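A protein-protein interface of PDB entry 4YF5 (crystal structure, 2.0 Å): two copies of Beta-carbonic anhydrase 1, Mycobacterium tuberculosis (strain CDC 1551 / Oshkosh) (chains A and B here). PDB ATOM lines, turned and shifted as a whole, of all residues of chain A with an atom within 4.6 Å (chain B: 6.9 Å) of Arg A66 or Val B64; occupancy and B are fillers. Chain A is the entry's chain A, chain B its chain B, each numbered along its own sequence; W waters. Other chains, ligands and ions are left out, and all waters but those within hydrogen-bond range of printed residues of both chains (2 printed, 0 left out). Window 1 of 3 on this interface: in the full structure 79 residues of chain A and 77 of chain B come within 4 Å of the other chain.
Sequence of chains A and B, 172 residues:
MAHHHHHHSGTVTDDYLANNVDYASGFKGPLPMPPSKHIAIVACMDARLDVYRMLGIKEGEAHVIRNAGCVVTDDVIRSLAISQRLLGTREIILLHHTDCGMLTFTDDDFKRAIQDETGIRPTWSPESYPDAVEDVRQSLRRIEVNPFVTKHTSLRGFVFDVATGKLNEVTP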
ATOM      1  N   ALA A  43     -27.318  15.355 -22.715  1.00  0.00           N
ATOM      2  CA  ALA A  43     -28.443  16.178 -22.314  1.00  0.00           C
ATOM      3  C   ALA A  43     -28.569  17.494 -23.088  1.00  0.00           C
ATOM      4  O   ALA A  43     -27.815  17.793 -23.994  1.00  0.00           O
ATOM      5  CB  ALA A  43     -28.362  16.481 -20.824  1.00  0.00           C
ATOM      6  N   CYS A  44     -29.563  18.272 -22.702  1.00  0.00           N
ATOM      7  CA  CYS A  44     -29.923  19.472 -23.419  1.00  0.00           C
ATOM      8  C   CYS A  44     -29.180  20.658 -22.843  1.00  0.00           C
ATOM      9  O   CYS A  44     -28.838  20.670 -21.668  1.00  0.00           O
ATOM     10  CB  CYS A  44     -31.427  19.660 -23.327  1.00  0.00           C
ATOM     11  SG  CYS A  44     -32.192  18.091 -22.850  1.00  0.00           S
ATOM     12  N   MET A  45     -28.929  21.662 -23.668  1.00  0.00           N
ATOM     13  CA  MET A  45     -28.318  22.885 -23.159  1.00  0.00           C
ATOM     14  C   MET A  45     -29.268  23.714 -22.294  1.00  0.00           C
ATOM     15  O   MET A  45     -28.830  24.662 -21.617  1.00  0.00           O
ATOM     16  CB  MET A  45     -27.826  23.735 -24.311  1.00  0.00           C
ATOM     17  CG  MET A  45     -28.938  24.417 -25.086  1.00  0.00           C
ATOM     18  SD  MET A  45     -28.180  25.316 -26.441  1.00  0.00           S
ATOM     19  CE  MET A  45     -29.612  26.136 -27.122  1.00  0.00           C
ATOM     20  N   ASP A  46     -30.553  23.359 -22.324  1.00  0.00           N
ATOM     21  CA  ASP A  46     -31.613  24.085 -21.604  1.00  0.00           C
ATOM     22  C   ASP A  46     -31.169  24.622 -20.236  1.00  0.00           C
ATOM     23  O   ASP A  46     -30.557  23.907 -19.434  1.00  0.00           O
ATOM     24  CB  ASP A  46     -32.841  23.189 -21.435  1.00  0.00           C
ATOM     25  CG  ASP A  46     -34.088  23.974 -21.018  1.00  0.00           C
ATOM     26  OD1 ASP A  46     -34.247  24.279 -19.821  1.00  0.00           O
ATOM     27  OD2 ASP A  46     -34.913  24.277 -21.892  1.00  0.00           O
ATOM     28  N   LEU A  49     -31.805  22.839 -16.738  1.00  0.00           N
ATOM     29  CA  LEU A  49     -31.258  21.533 -16.374  1.00  0.00           C
ATOM     30  C   LEU A  49     -29.855  21.682 -15.809  1.00  0.00           C
ATOM     31  O   LEU A  49     -28.882  21.845 -16.547  1.00  0.00           O
ATOM     32  CB  LEU A  49     -31.253  20.570 -17.570  1.00  0.00           C
ATOM     33  CG  LEU A  49     -32.575  19.898 -17.960  1.00  0.00           C
ATOM     34  CD1 LEU A  49     -33.662  20.916 -18.335  1.00  0.00           C
ATOM     35  CD2 LEU A  49     -32.344  18.901 -19.085  1.00  0.00           C
ATOM     36  N   VAL A  51     -27.698  19.458 -14.807  1.00  0.00           N
ATOM     37  CA  VAL A  51     -27.485  18.018 -14.936  1.00  0.00           C
ATOM     38  C   VAL A  51     -26.787  17.386 -13.724  1.00  0.00           C
ATOM     39  O   VAL A  51     -27.191  16.309 -13.256  1.00  0.00           O
ATOM     40  CB  VAL A  51     -26.682  17.706 -16.217  1.00  0.00           C
ATOM     41  CG1 VAL A  51     -26.281  16.224 -16.260  1.00  0.00           C
ATOM     42  CG2 VAL A  51     -27.497  18.070 -17.450  1.00  0.00           C
ATOM     43  N   VAL A  64     -20.313  14.735 -19.244  1.00  0.00           N
ATOM     44  CA  VAL A  64     -21.602  15.354 -19.551  1.00  0.00           C
ATOM     45  C   VAL A  64     -21.551  16.096 -20.877  1.00  0.00           C
ATOM     46  O   VAL A  64     -20.838  17.085 -21.011  1.00  0.00           O
ATOM     47  CB  VAL A  64     -22.061  16.348 -18.477  1.00  0.00           C
ATOM     48  CG1 VAL A  64     -23.318  17.037 -18.952  1.00  0.00           C
ATOM     49  CG2 VAL A  64     -22.300  15.631 -17.149  1.00  0.00           C
ATOM     50  N   ILE A  65     -22.335  15.608 -21.833  1.00  0.00           N
ATOM     51  CA  ILE A  65     -22.442  16.170 -23.181  1.00  0.00           C
ATOM     52  C   ILE A  65     -23.770  16.890 -23.298  1.00  0.00           C
ATOM     53  O   ILE A  65     -24.803  16.358 -22.865  1.00  0.00           O
ATOM     54  CB  ILE A  65     -22.363  15.066 -24.238  1.00  0.00           C
ATOM     55  CG1 ILE A  65     -21.014  14.341 -24.109  1.00  0.00           C
ATOM     56  CG2 ILE A  65     -22.602  15.613 -25.649  1.00  0.00           C
ATOM     57  CD1 ILE A  65     -21.043  12.909 -24.590  1.00  0.00           C
ATOM     58  N   ARG A  66     -23.759  18.084 -23.888  1.00  0.00           N
ATOM     59  CA  ARG A  66     -24.972  18.913 -23.968  1.00  0.00           C
ATOM     60  C   ARG A  66     -25.019  19.706 -25.274  1.00  0.00           C
ATOM     61  O   ARG A  66     -24.021  20.307 -25.673  1.00  0.00           O
ATOM     62  CB  ARG A  66     -25.060  19.892 -22.777  1.00  0.00           C
ATOM     63  CG  ARG A  66     -24.891  19.271 -21.398  1.00  0.00           C
ATOM     64  CD  ARG A  66     -25.019  20.288 -20.268  1.00  0.00           C
ATOM     65  NE  ARG A  66     -26.361  20.851 -20.211  1.00  0.00           N
ATOM     66  CZ  ARG A  66     -26.937  21.317 -19.109  1.00  0.00           C
ATOM     67  NH1 ARG A  66     -26.302  21.270 -17.943  1.00  0.00           N
ATOM     68  NH2 ARG A  66     -28.157  21.821 -19.177  1.00  0.00           N
ATOM     69  N   ASN A  67     -26.181  19.724 -25.922  1.00  0.00           N
ATOM     70  CA  ASN A  67     -26.402  20.579 -27.085  1.00  0.00           C
ATOM     71  C   ASN A  67     -27.866  21.028 -27.133  1.00  0.00           C
ATOM     72  O   ASN A  67     -28.640  20.690 -26.241  1.00  0.00           O
ATOM     73  CB  ASN A  67     -25.967  19.864 -28.385  1.00  0.00           C
ATOM     74  CG  ASN A  67     -26.789  18.624 -28.712  1.00  0.00           C
ATOM     75  OD1 ASN A  67     -27.851  18.386 -28.157  1.00  0.00           O
ATOM     76  ND2 ASN A  67     -26.290  17.835 -29.651  1.00  0.00           N
ATOM     77  N   ILE B  39     -26.939  34.230 -21.458  1.00  0.00           N
ATOM     78  CA  ILE B  39     -25.562  33.820 -21.705  1.00  0.00           C
ATOM     79  C   ILE B  39     -25.485  32.331 -22.075  1.00  0.00           C
ATOM     80  O   ILE B  39     -26.289  31.504 -21.603  1.00  0.00           O
ATOM     81  CB  ILE B  39     -24.671  34.117 -20.473  1.00  0.00           C
ATOM     82  CG1 ILE B  39     -23.210  33.743 -20.738  1.00  0.00           C
ATOM     83  CG2 ILE B  39     -25.203  33.413 -19.235  1.00  0.00           C
ATOM     84  CD1 ILE B  39     -22.267  34.185 -19.632  1.00  0.00           C
ATOM     85  N   ALA B  40     -24.546  32.004 -22.956  1.00  0.00           N
ATOM     86  CA  ALA B  40     -24.289  30.609 -23.318  1.00  0.00           C
ATOM     87  C   ALA B  40     -22.872  30.204 -22.958  1.00  0.00           C
ATOM     88  O   ALA B  40     -21.921  30.941 -23.212  1.00  0.00           O
ATOM     89  CB  ALA B  40     -24.535  30.384 -24.802  1.00  0.00           C
ATOM     90  N   ILE B  41     -22.735  29.028 -22.353  1.00  0.00           N
ATOM     91  CA  ILE B  41     -21.417  28.491 -22.088  1.00  0.00           C
ATOM     92  C   ILE B  41     -21.104  27.345 -23.039  1.00  0.00           C
ATOM     93  O   ILE B  41     -21.879  26.395 -23.170  1.00  0.00           O
ATOM     94  CB  ILE B  41     -21.269  27.980 -20.643  1.00  0.00           C
ATOM     95  CG1 ILE B  41     -22.018  28.880 -19.657  1.00  0.00           C
ATOM     96  CG2 ILE B  41     -19.789  27.865 -20.295  1.00  0.00           C
ATOM     97  CD1 ILE B  41     -21.369  30.226 -19.395  1.00  0.00           C
ATOM     98  N   VAL B  42     -19.969  27.447 -23.724  1.00  0.00           N
ATOM     99  CA  VAL B  42     -19.475  26.334 -24.513  1.00  0.00           C
ATOM    100  C   VAL B  42     -18.328  25.683 -23.752  1.00  0.00           C
ATOM    101  O   VAL B  42     -17.255  26.285 -23.589  1.00  0.00           O
ATOM    102  CB  VAL B  42     -18.996  26.773 -25.889  1.00  0.00           C
ATOM    103  CG1 VAL B  42     -18.479  25.566 -26.663  1.00  0.00           C
ATOM    104  CG2 VAL B  42     -20.116  27.459 -26.637  1.00  0.00           C
ATOM    105  N   ALA B  43     -18.549  24.461 -23.283  1.00  0.00           N
ATOM    106  CA  ALA B  43     -17.553  23.787 -22.454  1.00  0.00           C
ATOM    107  C   ALA B  43     -17.270  22.346 -22.881  1.00  0.00           C
ATOM    108  O   ALA B  43     -17.669  21.897 -23.948  1.00  0.00           O
ATOM    109  CB  ALA B  43     -17.984  23.818 -20.986  1.00  0.00           C
ATOM    110  N   MET B  45     -16.882  18.033 -22.046  1.00  0.00           N
ATOM    111  CA  MET B  45     -17.594  16.981 -21.341  1.00  0.00           C
ATOM    112  C   MET B  45     -16.779  16.520 -20.146  1.00  0.00           C
ATOM    113  O   MET B  45     -17.312  15.848 -19.255  1.00  0.00           O
ATOM    114  CB  MET B  45     -17.899  15.795 -22.271  1.00  0.00           C
ATOM    115  CG  MET B  45     -16.681  15.065 -22.765  1.00  0.00           C
ATOM    116  SD  MET B  45     -17.061  13.680 -23.903  1.00  0.00           S
ATOM    117  CE  MET B  45     -15.437  12.940 -24.048  1.00  0.00           C
ATOM    118  N   VAL B  51     -19.408  22.713 -14.559  1.00  0.00           N
ATOM    119  CA  VAL B  51     -19.533  24.051 -15.138  1.00  0.00           C
ATOM    120  C   VAL B  51     -20.433  24.978 -14.332  1.00  0.00           C
ATOM    121  O   VAL B  51     -20.118  26.151 -14.161  1.00  0.00           O
ATOM    122  CB  VAL B  51     -20.064  23.987 -16.592  1.00  0.00           C
ATOM    123  CG1 VAL B  51     -20.259  25.399 -17.154  1.00  0.00           C
ATOM    124  CG2 VAL B  51     -19.106  23.177 -17.464  1.00  0.00           C
ATOM    125  N   TYR B  52     -21.549  24.457 -13.835  1.00  0.00           N
ATOM    126  CA  TYR B  52     -22.447  25.260 -12.996  1.00  0.00           C
ATOM    127  C   TYR B  52     -21.756  25.813 -11.739  1.00  0.00           C
ATOM    128  O   TYR B  52     -21.899  26.988 -11.398  1.00  0.00           O
ATOM    129  CB  TYR B  52     -23.666  24.435 -12.576  1.00  0.00           C
ATOM    130  CG  TYR B  52     -24.897  24.651 -13.431  1.00  0.00           C
ATOM    131  CD1 TYR B  52     -24.911  24.294 -14.772  1.00  0.00           C
ATOM    132  CD2 TYR B  52     -26.052  25.197 -12.887  1.00  0.00           C
ATOM    133  CE1 TYR B  52     -26.041  24.489 -15.551  1.00  0.00           C
ATOM    134  CE2 TYR B  52     -27.184  25.391 -13.659  1.00  0.00           C
ATOM    135  CZ  TYR B  52     -27.174  25.036 -14.983  1.00  0.00           C
ATOM    136  OH  TYR B  52     -28.303  25.226 -15.743  1.00  0.00           O
ATOM    137  N   ILE B  57     -23.265  29.399 -11.353  1.00  0.00           N
ATOM    138  CA  ILE B  57     -24.489  29.420 -12.142  1.00  0.00           C
ATOM    139  C   ILE B  57     -25.675  28.889 -11.336  1.00  0.00           C
ATOM    140  O   ILE B  57     -25.543  27.904 -10.618  1.00  0.00           O
ATOM    141  CB  ILE B  57     -24.315  28.584 -13.440  1.00  0.00           C
ATOM    142  CG1 ILE B  57     -23.193  29.172 -14.298  1.00  0.00           C
ATOM    143  CG2 ILE B  57     -25.597  28.529 -14.234  1.00  0.00           C
ATOM    144  CD1 ILE B  57     -22.885  28.360 -15.526  1.00  0.00           C
ATOM    145  N   ALA B  62     -28.399  30.113 -17.583  1.00  0.00           N
ATOM    146  CA  ALA B  62     -27.456  29.985 -18.684  1.00  0.00           C
ATOM    147  C   ALA B  62     -27.634  28.725 -19.528  1.00  0.00           C
ATOM    148  O   ALA B  62     -27.937  27.638 -19.011  1.00  0.00           O
ATOM    149  CB  ALA B  62     -26.036  30.048 -18.136  1.00  0.00           C
ATOM    150  N   HIS B  63     -27.439  28.875 -20.832  1.00  0.00           N
ATOM    151  CA  HIS B  63     -27.289  27.707 -21.690  1.00  0.00           C
ATOM    152  C   HIS B  63     -25.908  27.154 -21.507  1.00  0.00           C
ATOM    153  O   HIS B  63     -24.930  27.911 -21.486  1.00  0.00           O
ATOM    154  CB  HIS B  63     -27.533  28.052 -23.152  1.00  0.00           C
ATOM    155  CG  HIS B  63     -28.981  28.130 -23.503  1.00  0.00           C
ATOM    156  ND1 HIS B  63     -29.456  28.865 -24.567  1.00  0.00           N
ATOM    157  CD2 HIS B  63     -30.063  27.551 -22.927  1.00  0.00           C
ATOM    158  CE1 HIS B  63     -30.770  28.743 -24.627  1.00  0.00           C
ATOM    159  NE2 HIS B  63     -31.163  27.954 -23.641  1.00  0.00           N
ATOM    160  N   VAL B  64     -25.820  25.831 -21.373  1.00  0.00           N
ATOM    161  CA  VAL B  64     -24.534  25.161 -21.250  1.00  0.00           C
ATOM    162  C   VAL B  64     -24.372  24.060 -22.303  1.00  0.00           C
ATOM    163  O   VAL B  64     -25.093  23.062 -22.296  1.00  0.00           O
ATOM    164  CB  VAL B  64     -24.339  24.563 -19.852  1.00  0.00           C
ATOM    165  CG1 VAL B  64     -22.966  23.914 -19.757  1.00  0.00           C
ATOM    166  CG2 VAL B  64     -24.496  25.656 -18.787  1.00  0.00           C
ATOM    167  N   ILE B  65     -23.419  24.275 -23.202  1.00  0.00           N
ATOM    168  CA  ILE B  65     -23.104  23.347 -24.283  1.00  0.00           C
ATOM    169  C   ILE B  65     -21.795  22.651 -23.930  1.00  0.00           C
ATOM    170  O   ILE B  65     -20.862  23.289 -23.441  1.00  0.00           O
ATOM    171  CB  ILE B  65     -22.982  24.088 -25.647  1.00  0.00           C
ATOM    172  CG1 ILE B  65     -24.289  24.838 -25.963  1.00  0.00           C
ATOM    173  CG2 ILE B  65     -22.608  23.112 -26.775  1.00  0.00           C
ATOM    174  CD1 ILE B  65     -24.132  26.014 -26.955  1.00  0.00           C
ATOM    175  N   ARG B  66     -21.729  21.344 -24.146  1.00  0.00           N
ATOM    176  CA  ARG B  66     -20.528  20.589 -23.806  1.00  0.00           C
ATOM    177  C   ARG B  66     -20.312  19.481 -24.817  1.00  0.00           C
ATOM    178  O   ARG B  66     -21.252  18.761 -25.179  1.00  0.00           O
ATOM    179  CB  ARG B  66     -20.623  19.989 -22.381  1.00  0.00           C
ATOM    180  CG  ARG B  66     -20.793  21.001 -21.258  1.00  0.00           C
ATOM    181  CD  ARG B  66     -21.033  20.365 -19.866  1.00  0.00           C
ATOM    182  NE  ARG B  66     -19.794  19.814 -19.338  1.00  0.00           N
ATOM    183  CZ  ARG B  66     -19.512  19.647 -18.051  1.00  0.00           C
ATOM    184  NH1 ARG B  66     -20.378  19.987 -17.104  1.00  0.00           N
ATOM    185  NH2 ARG B  66     -18.339  19.140 -17.715  1.00  0.00           N
ATOM    186  N   ASN B  67     -19.068  19.311 -25.243  1.00  0.00           N
ATOM    187  CA  ASN B  67     -18.719  18.148 -26.037  1.00  0.00           C
ATOM    188  C   ASN B  67     -17.291  17.755 -25.741  1.00  0.00           C
ATOM    189  O   ASN B  67     -16.650  18.354 -24.868  1.00  0.00           O
ATOM    190  CB  ASN B  67     -18.930  18.430 -27.531  1.00  0.00           C
ATOM    191  CG  ASN B  67     -18.031  19.545 -28.052  1.00  0.00           C
ATOM    192  OD1 ASN B  67     -17.111  19.997 -27.370  1.00  0.00           O
ATOM    193  ND2 ASN B  67     -18.304  19.993 -29.271  1.00  0.00           N
ATOM    194  N   ASP B  75     -22.273  21.414 -34.602  1.00  0.00           N
ATOM    195  CA  ASP B  75     -23.339  21.173 -33.636  1.00  0.00           C
ATOM    196  C   ASP B  75     -23.346  22.297 -32.613  1.00  0.00           C
ATOM    197  O   ASP B  75     -24.411  22.760 -32.174  1.00  0.00           O
ATOM    198  CB  ASP B  75     -23.173  19.807 -32.970  1.00  0.00           C
ATOM    199  CG  ASP B  75     -24.373  19.419 -32.072  1.00  0.00           C
ATOM    200  OD1 ASP B  75     -25.425  20.095 -32.089  1.00  0.00           O
ATOM    201  OD2 ASP B  75     -24.248  18.415 -31.347  1.00  0.00           O
ATOM    202  N   VAL B  76     -22.157  22.777 -32.261  1.00  0.00           N
ATOM    203  CA  VAL B  76     -22.062  23.909 -31.337  1.00  0.00           C
ATOM    204  C   VAL B  76     -22.573  25.210 -31.986  1.00  0.00           C
ATOM    205  O   VAL B  76     -23.258  26.013 -31.344  1.00  0.00           O
ATOM    206  CB  VAL B  76     -20.619  24.091 -30.839  1.00  0.00           C
ATOM    207  CG1 VAL B  76     -20.478  25.372 -30.045  1.00  0.00           C
ATOM    208  CG2 VAL B  76     -20.211  22.889 -29.978  1.00  0.00           C
ATOM    209  N   SER B  79     -26.298  25.051 -31.986  1.00  0.00           N
ATOM    210  CA  SER B  79     -26.835  25.259 -30.663  1.00  0.00           C
ATOM    211  C   SER B  79     -26.727  26.739 -30.266  1.00  0.00           C
ATOM    212  O   SER B  79     -27.644  27.271 -29.644  1.00  0.00           O
ATOM    213  CB  SER B  79     -26.128  24.333 -29.661  1.00  0.00           C
ATOM    214  OG  SER B  79     -26.240  22.980 -30.104  1.00  0.00           O
HETATM  215  O   HOH W   1     -33.416  27.129 -22.056  1.00  0.00           O
HETATM  216  O   HOH W   2     -27.968  24.890 -18.175  1.00  0.00           O
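N of Ala A43 sits at hydrogen-bond distance from O of Ile A65 (2.7 Å). O of Ile B39 is in hydrogen-bond range of N of His B63 (3.0 Å). The backbone carbonyl oxygen (O) of His B63 is in hydrogen-bond range of the backbone NH (N) of Ile B41 (2.6 Å). N of Met B45 is in hydrogen-bond range of O of Asn B67 (2.8 Å). N of Ile B57 is in hydrogen-bond range of O of Tyr B52 (2.8 Å). The side-chain hydroxyl (OG) of Ser B79 is in hydrogen-bond range of the backbone carbonyl oxygen (O) of Asp B75 (2.8 Å).
Of the printed residues of chain B, Arg A66 touches Val B64 (3.2 Å), Ile B65 (3.3 Å) and Arg B66 (2.9 Å). Of the printed residues of chain A, Met B45 touches Val A64 and Ile A65. Of the printed residues of chain A, Asp B75 touches Asn A67 (2.7 Å). Printed residues of chain B within 4 Å of Asn A67: Asp B75 and Ser B79. Printed residues of chain A within 4 Å of Tyr B52: Leu A49. The nearest printed residue of chain B that does not touch Arg A66 is Tyr B52 (4.02 Å). The nearest printed residue of chain A that does not touch Met B45 is Arg A66 (6.5 Å).
Water W2 lies within hydrogen-bond range of OH of Tyr B52 (2.5 Å), O of Ala B62 (2.9 Å), O of Asp A46 (3.0 Å) and NH2 of Arg A66 (3.2 Å). Water W1 lies within hydrogen-bond range of NE2 of His B63 (2.9 Å) and OD2 of Asp A46 (3.2 Å).
The backbone carbonyl oxygen (O) of Met A45 is in hydrogen-bond range of the backbone NH (N) of Val B64. The backbone NH of Val A64 is in hydrogen-bond range of the backbone carbonyl oxygen of Met B45, 3.2 Å away. The backbone carbonyl oxygen of Val A64 sits close to the guanidinium group of Arg B66. The backbone carbonyl oxygen of Val B64 sits close to the guanidinium group of Arg A66 (3.3 Å). O of Arg B66 sits at hydrogen-bond distance from N of Arg A66, 2.9 Å away. The side-chain amide nitrogen of Asn A67 sits at hydrogen-bond distance from the side-chain carboxylate of Asp B75 (2.7 Å). SD of Met A45 lies close to O of Ser B79, 3.8 Å away.
Met A45 touches Val B64, and with the chains exchanged Val A64 touches Met B45. Met A45 touches Ile B65, and with the chains exchanged Ile A65 touches Met B45. Val A64 touches Arg B66, and with the chains exchanged Arg A66 touches Val B64. Arg B66 touches its own counterpart, Arg A66. Of the 14 pairs that touch across the chains among the printed residues, 9 have their exchanged pair printed and touching as well.
Hydrophobic or aromatic side chains of chain A that line the printed part of chain B: Met A45 and Ile A65. Of the 18 printed residues of chain B, 8 touch a printed residue of chain A. Among the printed residues, no Asp or Glu carboxylate lies within 4 Å of a Lys or Arg side-chain nitrogen of the other chain.
Among the printed residues, pairs that only touch across the chains: Arg A66 with Ile B65, Met A45 with His B63, Ile A65 with Arg B66, Leu A49 with Tyr B52, Asn A67 with Ser B79, Ile A65 with Met B45 and Met A45 with Ile B65.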
